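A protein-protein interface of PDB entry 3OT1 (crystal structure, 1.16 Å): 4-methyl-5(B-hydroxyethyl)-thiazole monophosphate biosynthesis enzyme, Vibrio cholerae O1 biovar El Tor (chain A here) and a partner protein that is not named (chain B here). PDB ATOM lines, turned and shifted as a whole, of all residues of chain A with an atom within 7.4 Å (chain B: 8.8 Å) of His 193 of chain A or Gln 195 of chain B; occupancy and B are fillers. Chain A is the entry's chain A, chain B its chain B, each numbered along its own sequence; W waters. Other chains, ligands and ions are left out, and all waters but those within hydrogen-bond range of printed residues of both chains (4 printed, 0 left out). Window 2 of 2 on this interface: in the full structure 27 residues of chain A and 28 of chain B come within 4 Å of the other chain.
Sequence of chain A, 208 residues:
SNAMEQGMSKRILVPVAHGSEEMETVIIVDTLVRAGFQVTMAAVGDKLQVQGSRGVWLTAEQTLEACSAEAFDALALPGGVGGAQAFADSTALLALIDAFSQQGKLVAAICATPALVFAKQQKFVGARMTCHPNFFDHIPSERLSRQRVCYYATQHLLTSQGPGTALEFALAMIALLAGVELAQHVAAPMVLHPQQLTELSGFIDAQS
The backbone NH (N) of His 193 of chain A lies close to the guanidinium group (NH2) of Arg 148 of chain B, 3.4 Å away. The backbone carbonyl oxygen (O) of Met 190 of chain A is in hydrogen-bond range of the backbone NH (N) of Gly 164 of chain B. NH1 of Arg 148 of chain B sits at hydrogen-bond distance from O of Leu 192 of chain A (3.1 Å). NH2 of Arg 148 of chain B sits at hydrogen-bond distance from O of Val 191 of chain A (3.0 Å).
Water W2 lies within hydrogen-bond range of OE2 of Glu 199 of chain A (2.6 Å), NE2 of His 193 of chain B (2.8 Å) and OE1 of Gln 195 of chain A (2.9 Å). Water W3 lies within hydrogen-bond range of OE1 of Gln 196 of chain B and NE2 of Gln 196 of chain A. Water W4 lies within hydrogen-bond range of the side-chain amide oxygen (OE1) of Gln 196 of chain A (2.7 Å), the backbone carbonyl oxygen (O) of Gly 164 of chain B (2.8 Å) and the side-chain amide nitrogen (NE2) of Gln 196 of chain B (3.4 Å). Water W1 lies within hydrogen-bond range of O of Gln 195 of chain B (2.8 Å) and NE2 of His 193 of chain A (2.9 Å).
Pro 163 of chain B touches Met 190 of chain A (N to O, 3.7 Å). Val 191 of chain A touches Gly 164 of chain B (O to C, 3.4 Å). CG2 of Thr 165 of chain B touches CG1 of Val 191 of chain A (3.7 Å). His 193 of chain A touches Gln 195 of chain B (NE2 to CB, 3.5 Å). NE2 of His 193 of chain B touches CB of Gln 195 of chain A, 3.5 Å away. NE2 of Gln 196 of chain A touches OE1 of Gln 196 of chain B, 3.7 Å away.
Printed residues of chain B within 4 Å of Leu 192 of chain A: Arg 148 (3.1 Å). His 193 of chain A touches just these residues of chain B: Arg 148 and Gln 195. Pro 194 of chain A touches none of the printed residues of chain B. Printed residues of chain A within 4 Å of Arg 148 of chain B: Val 191 (3.0 Å), Leu 192 (3.1 Å) and His 193 (3.4 Å). Of the printed residues of chain A, Gly 164 of chain B touches Met 190 (2.7 Å) and Val 191 (3.4 Å). Gln 195 of chain B touches just one residue of chain A: His 193. Printed residues of chain A within 4 Å of Gln 196 of chain B: Gln 196. The nearest residue of chain B that does not touch His 193 of chain A is Gln 196 of chain B (4.1 Å). The nearest printed residue of chain B that does not touch Gln 196 of chain A is His 193 of chain B (4.6 Å).
Hydrophobic or aromatic side chains of chain A within 4 Å of the printed part of chain B: Val 191 and His 193. Of the 15 printed residues of chain B, 7 touch a printed residue of chain A. Printed residues of chain B that touch a printed residue of chain A: Arg 148, Pro 163, Gly 164, Thr 165, His 193, Gln 195 and Gln 196. Hydrophobic or aromatic side chains of chain B that line the printed part of chain A: Pro 163 and His 193. Among the printed residues, no Asp or Glu carboxylate lies within 4 Å of a Lys or Arg side-chain nitrogen of the other chain.
N of His 193 of chain B is in hydrogen-bond range of OE1 of Gln 196 of chain B (3.0 Å). The backbone NH (N) of Gln 195 of chain A sits at hydrogen-bond distance from a ring nitrogen (ND1) of His 193 of chain A (3.0 Å). The side-chain carboxylate (OE2) of Glu 168 of chain B sits at hydrogen-bond distance from the side-chain amide nitrogen (NE2) of Gln 196 of chain B, 2.9 Å away. O of Gly 164 of chain B sits at hydrogen-bond distance from NH2 of Arg 148 of chain B, at 3.0 Å. The backbone NH (N) of His 193 of chain A lies within hydrogen-bond range of the side-chain amide oxygen (OE1) of Gln 196 of chain A, 2.9 Å away. NE of Arg 148 of chain B is in salt-bridge range of OE1 of Glu 168 of chain B, 2.8 Å away.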
ATOM      1  N   LEU A 167      -9.689  23.401 -15.103  1.00  0.00           N
ATOM      2  CA  LEU A 167      -9.542  24.830 -14.911  1.00  0.00           C
ATOM      3  C   LEU A 167     -10.478  25.338 -13.796  1.00  0.00           C
ATOM      4  O   LEU A 167     -10.077  26.098 -12.910  1.00  0.00           O
ATOM      5  CB  LEU A 167      -9.799  25.510 -16.234  1.00  0.00           C
ATOM      6  CG  LEU A 167      -9.592  27.000 -16.296  1.00  0.00           C
ATOM      7  CD1 LEU A 167      -8.292  27.396 -15.654  1.00  0.00           C
ATOM      8  CD2 LEU A 167      -9.662  27.474 -17.755  1.00  0.00           C
ATOM      9  N   MET A 190      -8.242  33.913 -18.976  1.00  0.00           N
ATOM     10  CA  MET A 190      -8.087  32.610 -19.431  1.00  0.00           C
ATOM     11  C   MET A 190      -9.165  32.237 -20.464  1.00  0.00           C
ATOM     12  O   MET A 190      -9.070  31.179 -21.049  1.00  0.00           O
ATOM     13  CB  MET A 190      -7.950  31.738 -18.211  1.00  0.00           C
ATOM     14  CG  MET A 190      -6.826  32.253 -17.315  1.00  0.00           C
ATOM     15  SD  MET A 190      -6.568  31.070 -15.853  1.00  0.00           S
ATOM     16  CE  MET A 190      -5.717  29.613 -16.785  1.00  0.00           C
ATOM     17  N   VAL A 191     -10.131  33.126 -20.737  1.00  0.00           N
ATOM     18  CA  VAL A 191     -11.179  32.910 -21.765  1.00  0.00           C
ATOM     19  C   VAL A 191     -11.975  31.647 -21.426  1.00  0.00           C
ATOM     20  O   VAL A 191     -12.249  30.789 -22.263  1.00  0.00           O
ATOM     21  CB  VAL A 191     -10.657  32.917 -23.242  1.00  0.00           C
ATOM     22  CG1 VAL A 191     -11.797  33.230 -24.181  1.00  0.00           C
ATOM     23  CG2 VAL A 191      -9.527  33.942 -23.407  1.00  0.00           C
ATOM     24  N   LEU A 192     -12.368  31.550 -20.152  1.00  0.00           N
ATOM     25  CA  LEU A 192     -13.340  30.550 -19.725  1.00  0.00           C
ATOM     26  C   LEU A 192     -14.626  30.731 -20.509  1.00  0.00           C
ATOM     27  O   LEU A 192     -14.932  31.819 -20.973  1.00  0.00           O
ATOM     28  CB  LEU A 192     -13.679  30.708 -18.237  1.00  0.00           C
ATOM     29  CG  LEU A 192     -12.716  30.119 -17.211  1.00  0.00           C
ATOM     30  CD1 LEU A 192     -11.379  30.822 -17.187  1.00  0.00           C
ATOM     31  CD2 LEU A 192     -13.387  30.148 -15.843  1.00  0.00           C
ATOM     32  N   HIS A 193     -15.394  29.649 -20.584  1.00  0.00           N
ATOM     33  CA  HIS A 193     -16.738  29.757 -21.063  1.00  0.00           C
ATOM     34  C   HIS A 193     -17.464  30.662 -20.059  1.00  0.00           C
ATOM     35  O   HIS A 193     -17.230  30.579 -18.852  1.00  0.00           O
ATOM     36  CB  HIS A 193     -17.419  28.377 -21.146  1.00  0.00           C
ATOM     37  CG  HIS A 193     -18.780  28.428 -21.765  1.00  0.00           C
ATOM     38  ND1 HIS A 193     -19.892  28.841 -21.070  1.00  0.00           N
ATOM     39  CD2 HIS A 193     -19.189  28.196 -23.034  1.00  0.00           C
ATOM     40  CE1 HIS A 193     -20.934  28.849 -21.882  1.00  0.00           C
ATOM     41  NE2 HIS A 193     -20.536  28.449 -23.081  1.00  0.00           N
ATOM     42  N   PRO A 194     -18.371  31.527 -20.526  1.00  0.00           N
ATOM     43  CA  PRO A 194     -19.098  32.413 -19.621  1.00  0.00           C
ATOM     44  C   PRO A 194     -19.726  31.721 -18.401  1.00  0.00           C
ATOM     45  O   PRO A 194     -19.678  32.306 -17.296  1.00  0.00           O
ATOM     46  CB  PRO A 194     -20.160  33.008 -20.535  1.00  0.00           C
ATOM     47  CG  PRO A 194     -19.408  33.140 -21.816  1.00  0.00           C
ATOM     48  CD  PRO A 194     -18.665  31.850 -21.934  1.00  0.00           C
ATOM     49  N   GLN A 195     -20.213  30.487 -18.570  1.00  0.00           N
ATOM     50  CA  GLN A 195     -20.800  29.747 -17.468  1.00  0.00           C
ATOM     51  C   GLN A 195     -19.765  29.387 -16.425  1.00  0.00           C
ATOM     52  O   GLN A 195     -20.046  29.434 -15.213  1.00  0.00           O
ATOM     53  CB  GLN A 195     -21.516  28.473 -17.952  1.00  0.00           C
ATOM     54  CG  GLN A 195     -22.875  28.740 -18.593  1.00  0.00           C
ATOM     55  CD  GLN A 195     -23.874  29.265 -17.568  1.00  0.00           C
ATOM     56  OE1 GLN A 195     -24.208  28.567 -16.608  1.00  0.00           O
ATOM     57  NE2 GLN A 195     -24.330  30.502 -17.732  1.00  0.00           N
ATOM     58  N   GLN A 196     -18.571  28.998 -16.886  1.00  0.00           N
ATOM     59  CA  GLN A 196     -17.476  28.686 -15.967  1.00  0.00           C
ATOM     60  C   GLN A 196     -17.140  29.926 -15.125  1.00  0.00           C
ATOM     61  O   GLN A 196     -16.896  29.860 -13.920  1.00  0.00           O
ATOM     62  CB  GLN A 196     -16.278  28.125 -16.714  1.00  0.00           C
ATOM     63  CG  GLN A 196     -16.559  26.764 -17.406  1.00  0.00           C
ATOM     64  CD  GLN A 196     -15.441  26.352 -18.360  1.00  0.00           C
ATOM     65  OE1 GLN A 196     -14.943  27.162 -19.137  1.00  0.00           O
ATOM     66  NE2 GLN A 196     -15.016  25.072 -18.284  1.00  0.00           N
ATOM     67  N   LEU A 197     -17.032  31.064 -15.773  1.00  0.00           N
ATOM     68  CA  LEU A 197     -16.653  32.279 -15.049  1.00  0.00           C
ATOM     69  C   LEU A 197     -17.688  32.692 -14.000  1.00  0.00           C
ATOM     70  O   LEU A 197     -17.352  33.028 -12.855  1.00  0.00           O
ATOM     71  CB  LEU A 197     -16.367  33.424 -16.034  1.00  0.00           C
ATOM     72  CG  LEU A 197     -15.807  34.706 -15.409  1.00  0.00           C
ATOM     73  CD1 LEU A 197     -14.423  34.478 -14.796  1.00  0.00           C
ATOM     74  CD2 LEU A 197     -15.702  35.824 -16.430  1.00  0.00           C
ATOM     75  N   THR A 198     -18.963  32.636 -14.373  1.00  0.00           N
ATOM     76  CA  THR A 198     -20.040  32.931 -13.434  1.00  0.00           C
ATOM     77  C   THR A 198     -20.025  32.049 -12.188  1.00  0.00           C
ATOM     78  O   THR A 198     -20.209  32.513 -11.054  1.00  0.00           O
ATOM     79  CB  THR A 198     -21.367  32.788 -14.170  1.00  0.00           C
ATOM     80  OG1 THR A 198     -21.446  33.826 -15.147  1.00  0.00           O
ATOM     81  CG2 THR A 198     -22.531  32.871 -13.233  1.00  0.00           C
ATOM     82  N   GLU A 199     -19.760  30.779 -12.393  1.00  0.00           N
ATOM     83  CA  GLU A 199     -19.765  29.835 -11.300  1.00  0.00           C
ATOM     84  C   GLU A 199     -18.558  30.008 -10.395  1.00  0.00           C
ATOM     85  O   GLU A 199     -18.651  29.777  -9.201  1.00  0.00           O
ATOM     86  CB  GLU A 199     -19.881  28.431 -11.850  1.00  0.00           C
ATOM     87  CG  GLU A 199     -21.248  28.238 -12.468  1.00  0.00           C
ATOM     88  CD  GLU A 199     -21.509  26.854 -12.966  1.00  0.00           C
ATOM     89  OE1 GLU A 199     -20.628  25.951 -12.897  1.00  0.00           O
ATOM     90  OE2 GLU A 199     -22.623  26.681 -13.469  1.00  0.00           O
ATOM     91  N   ARG B 148     -14.838  32.008 -30.238  1.00  0.00           N
ATOM     92  CA  ARG B 148     -13.877  31.269 -29.426  1.00  0.00           C
ATOM     93  C   ARG B 148     -12.932  30.445 -30.271  1.00  0.00           C
ATOM     94  O   ARG B 148     -11.741  30.345 -29.933  1.00  0.00           O
ATOM     95  CB  ARG B 148     -14.609  30.383 -28.411  1.00  0.00           C
ATOM     96  CG  ARG B 148     -15.345  31.188 -27.362  1.00  0.00           C
ATOM     97  CD  ARG B 148     -16.216  30.335 -26.485  1.00  0.00           C
ATOM     98  NE  ARG B 148     -15.438  29.479 -25.586  1.00  0.00           N
ATOM     99  CZ  ARG B 148     -14.912  29.880 -24.432  1.00  0.00           C
ATOM    100  NH1 ARG B 148     -15.059  31.119 -23.987  1.00  0.00           N
ATOM    101  NH2 ARG B 148     -14.258  29.006 -23.690  1.00  0.00           N
ATOM    102  N   PRO B 163      -6.307  29.736 -22.984  1.00  0.00           N
ATOM    103  CA  PRO B 163      -6.317  28.463 -22.251  1.00  0.00           C
ATOM    104  C   PRO B 163      -7.704  27.825 -22.124  1.00  0.00           C
ATOM    105  O   PRO B 163      -7.846  26.611 -22.288  1.00  0.00           O
ATOM    106  CB  PRO B 163      -5.717  28.842 -20.899  1.00  0.00           C
ATOM    107  CG  PRO B 163      -4.818  30.014 -21.231  1.00  0.00           C
ATOM    108  CD  PRO B 163      -5.567  30.787 -22.257  1.00  0.00           C
ATOM    109  N   GLY B 164      -8.703  28.669 -21.865  1.00  0.00           N
ATOM    110  CA  GLY B 164     -10.070  28.209 -21.687  1.00  0.00           C
ATOM    111  C   GLY B 164     -10.797  27.820 -22.950  1.00  0.00           C
ATOM    112  O   GLY B 164     -11.917  27.325 -22.880  1.00  0.00           O
ATOM    113  N   THR B 165     -10.173  28.072 -24.112  1.00  0.00           N
ATOM    114  CA  THR B 165     -10.695  27.607 -25.388  1.00  0.00           C
ATOM    115  C   THR B 165      -9.833  26.509 -26.012  1.00  0.00           C
ATOM    116  O   THR B 165     -10.147  26.035 -27.106  1.00  0.00           O
ATOM    117  CB  THR B 165     -10.841  28.767 -26.422  1.00  0.00           C
ATOM    118  OG1 THR B 165      -9.561  29.219 -26.865  1.00  0.00           O
ATOM    119  CG2 THR B 165     -11.640  29.921 -25.900  1.00  0.00           C
ATOM    120  N   GLU B 168     -11.681  23.172 -26.818  1.00  0.00           N
ATOM    121  CA  GLU B 168     -12.547  23.407 -27.960  1.00  0.00           C
ATOM    122  C   GLU B 168     -11.752  23.446 -29.261  1.00  0.00           C
ATOM    123  O   GLU B 168     -12.160  22.897 -30.269  1.00  0.00           O
ATOM    124  CB  GLU B 168     -13.301  24.728 -27.785  1.00  0.00           C
ATOM    125  CG  GLU B 168     -14.312  24.726 -26.648  1.00  0.00           C
ATOM    126  CD  GLU B 168     -14.539  26.117 -26.109  1.00  0.00           C
ATOM    127  OE1 GLU B 168     -15.095  26.976 -26.839  1.00  0.00           O
ATOM    128  OE2 GLU B 168     -14.187  26.392 -24.939  1.00  0.00           O
ATOM    129  N   VAL B 191     -15.644  15.500 -19.834  1.00  0.00           N
ATOM    130  CA  VAL B 191     -16.372  16.392 -18.944  1.00  0.00           C
ATOM    131  C   VAL B 191     -16.227  17.858 -19.333  1.00  0.00           C
ATOM    132  O   VAL B 191     -16.063  18.751 -18.484  1.00  0.00           O
ATOM    133  CB  VAL B 191     -16.064  16.160 -17.425  1.00  0.00           C
ATOM    134  CG1 VAL B 191     -17.239  16.604 -16.587  1.00  0.00           C
ATOM    135  CG2 VAL B 191     -15.719  14.690 -17.124  1.00  0.00           C
ATOM    136  N   LEU B 192     -16.301  18.126 -20.631  1.00  0.00           N
ATOM    137  CA  LEU B 192     -16.536  19.454 -21.172  1.00  0.00           C
ATOM    138  C   LEU B 192     -17.769  20.052 -20.515  1.00  0.00           C
ATOM    139  O   LEU B 192     -18.681  19.300 -20.128  1.00  0.00           O
ATOM    140  CB  LEU B 192     -16.821  19.362 -22.686  1.00  0.00           C
ATOM    141  CG  LEU B 192     -15.676  19.125 -23.684  1.00  0.00           C
ATOM    142  CD1 LEU B 192     -14.898  17.823 -23.475  1.00  0.00           C
ATOM    143  CD2 LEU B 192     -16.220  19.152 -25.111  1.00  0.00           C
ATOM    144  N   HIS B 193     -17.877  21.370 -20.433  1.00  0.00           N
ATOM    145  CA  HIS B 193     -19.155  21.957 -20.111  1.00  0.00           C
ATOM    146  C   HIS B 193     -20.091  21.654 -21.287  1.00  0.00           C
ATOM    147  O   HIS B 193     -19.681  21.736 -22.438  1.00  0.00           O
ATOM    148  CB  HIS B 193     -19.006  23.472 -19.912  1.00  0.00           C
ATOM    149  CG  HIS B 193     -20.221  24.097 -19.301  1.00  0.00           C
ATOM    150  ND1 HIS B 193     -21.366  24.357 -20.024  1.00  0.00           N
ATOM    151  CD2 HIS B 193     -20.480  24.483 -18.026  1.00  0.00           C
ATOM    152  CE1 HIS B 193     -22.274  24.877 -19.222  1.00  0.00           C
ATOM    153  NE2 HIS B 193     -21.769  24.953 -18.002  1.00  0.00           N
ATOM    154  N   PRO B 194     -21.361  21.265 -21.034  1.00  0.00           N
ATOM    155  CA  PRO B 194     -22.262  20.959 -22.158  1.00  0.00           C
ATOM    156  C   PRO B 194     -22.282  22.049 -23.245  1.00  0.00           C
ATOM    157  O   PRO B 194     -22.370  21.752 -24.442  1.00  0.00           O
ATOM    158  CB  PRO B 194     -23.620  20.769 -21.477  1.00  0.00           C
ATOM    159  CG  PRO B 194     -23.277  20.253 -20.153  1.00  0.00           C
ATOM    160  CD  PRO B 194     -22.004  20.950 -19.753  1.00  0.00           C
ATOM    161  N   GLN B 195     -22.162  23.306 -22.851  1.00  0.00           N
ATOM    162  CA  GLN B 195     -22.234  24.389 -23.816  1.00  0.00           C
ATOM    163  C   GLN B 195     -20.950  24.525 -24.619  1.00  0.00           C
ATOM    164  O   GLN B 195     -20.987  25.135 -25.677  1.00  0.00           O
ATOM    165  CB  GLN B 195     -22.648  25.692 -23.114  1.00  0.00           C
ATOM    166  CG  GLN B 195     -24.025  25.639 -22.429  1.00  0.00           C
ATOM    167  CD  GLN B 195     -25.113  25.014 -23.283  1.00  0.00           C
ATOM    168  OE1 GLN B 195     -25.888  24.189 -22.790  1.00  0.00           O
ATOM    169  NE2 GLN B 195     -25.180  25.385 -24.551  1.00  0.00           N
ATOM    170  N   GLN B 196     -19.850  23.919 -24.183  1.00  0.00           N
ATOM    171  CA  GLN B 196     -18.618  23.922 -24.975  1.00  0.00           C
ATOM    172  C   GLN B 196     -18.644  22.970 -26.147  1.00  0.00           C
ATOM    173  O   GLN B 196     -17.746  23.029 -27.017  1.00  0.00           O
ATOM    174  CB  GLN B 196     -17.397  23.587 -24.109  1.00  0.00           C
ATOM    175  CG  GLN B 196     -17.008  24.691 -23.208  1.00  0.00           C
ATOM    176  CD  GLN B 196     -15.861  24.277 -22.329  1.00  0.00           C
ATOM    177  OE1 GLN B 196     -15.996  23.391 -21.479  1.00  0.00           O
ATOM    178  NE2 GLN B 196     -14.720  24.888 -22.537  1.00  0.00           N
ATOM    179  N   LEU B 197     -19.630  22.072 -26.150  1.00  0.00           N
ATOM    180  CA  LEU B 197     -19.788  20.994 -27.129  1.00  0.00           C
ATOM    181  C   LEU B 197     -20.862  21.248 -28.176  1.00  0.00           C
ATOM    182  O   LEU B 197     -21.138  20.363 -28.989  1.00  0.00           O
ATOM    183  CB  LEU B 197     -20.256  19.742 -26.397  1.00  0.00           C
ATOM    184  CG  LEU B 197     -19.269  18.758 -25.775  1.00  0.00           C
ATOM    185  CD1 LEU B 197     -19.878  18.203 -24.503  1.00  0.00           C
ATOM    186  CD2 LEU B 197     -18.942  17.631 -26.745  1.00  0.00           C
ATOM    187  N   THR B 198     -21.655  22.346 -28.004  1.00  0.00           N
ATOM    188  CA  THR B 198     -22.702  22.701 -28.966  1.00  0.00           C
ATOM    189  C   THR B 198     -22.275  23.093 -30.411  1.00  0.00           C
ATOM    190  O   THR B 198     -23.020  22.847 -31.342  1.00  0.00           O
ATOM    191  CB  THR B 198     -23.628  23.733 -28.335  1.00  0.00           C
ATOM    192  OG1 THR B 198     -24.020  23.225 -27.063  1.00  0.00           O
ATOM    193  CG2 THR B 198     -24.852  23.898 -29.133  1.00  0.00           C
ATOM    194  N   GLU B 199     -21.110  23.696 -30.624  1.00  0.00           N
ATOM    195  CA  GLU B 199     -20.695  24.040 -31.996  1.00  0.00           C
ATOM    196  C   GLU B 199     -19.641  23.104 -32.604  1.00  0.00           C
ATOM    197  O   GLU B 199     -19.321  23.197 -33.792  1.00  0.00           O
ATOM    198  CB  GLU B 199     -20.165  25.467 -32.064  1.00  0.00           C
ATOM    199  N   LEU B 200     -19.137  22.186 -31.791  1.00  0.00           N
ATOM    200  CA  LEU B 200     -18.129  21.244 -32.239  1.00  0.00           C
ATOM    201  C   LEU B 200     -18.812  20.649 -33.430  1.00  0.00           C
ATOM    202  O   LEU B 200     -18.199  20.214 -34.407  1.00  0.00           O
ATOM    203  CB  LEU B 200     -17.896  20.171 -31.182  1.00  0.00           C
ATOM    204  CG  LEU B 200     -17.133  18.942 -31.670  1.00  0.00           C
ATOM    205  CD1 LEU B 200     -15.844  19.383 -32.335  1.00  0.00           C
ATOM    206  CD2 LEU B 200     -16.862  17.989 -30.526  1.00  0.00           C
HETATM  207  O   HOH W   1     -21.589  27.901 -25.725  1.00  0.00           O
HETATM  208  O   HOH W   2     -23.325  25.944 -15.910  1.00  0.00           O
HETATM  209  O   HOH W   3     -13.742  22.732 -20.152  1.00  0.00           O
HETATM  210  O   HOH W   4     -12.625  26.395 -20.369  1.00  0.00           O
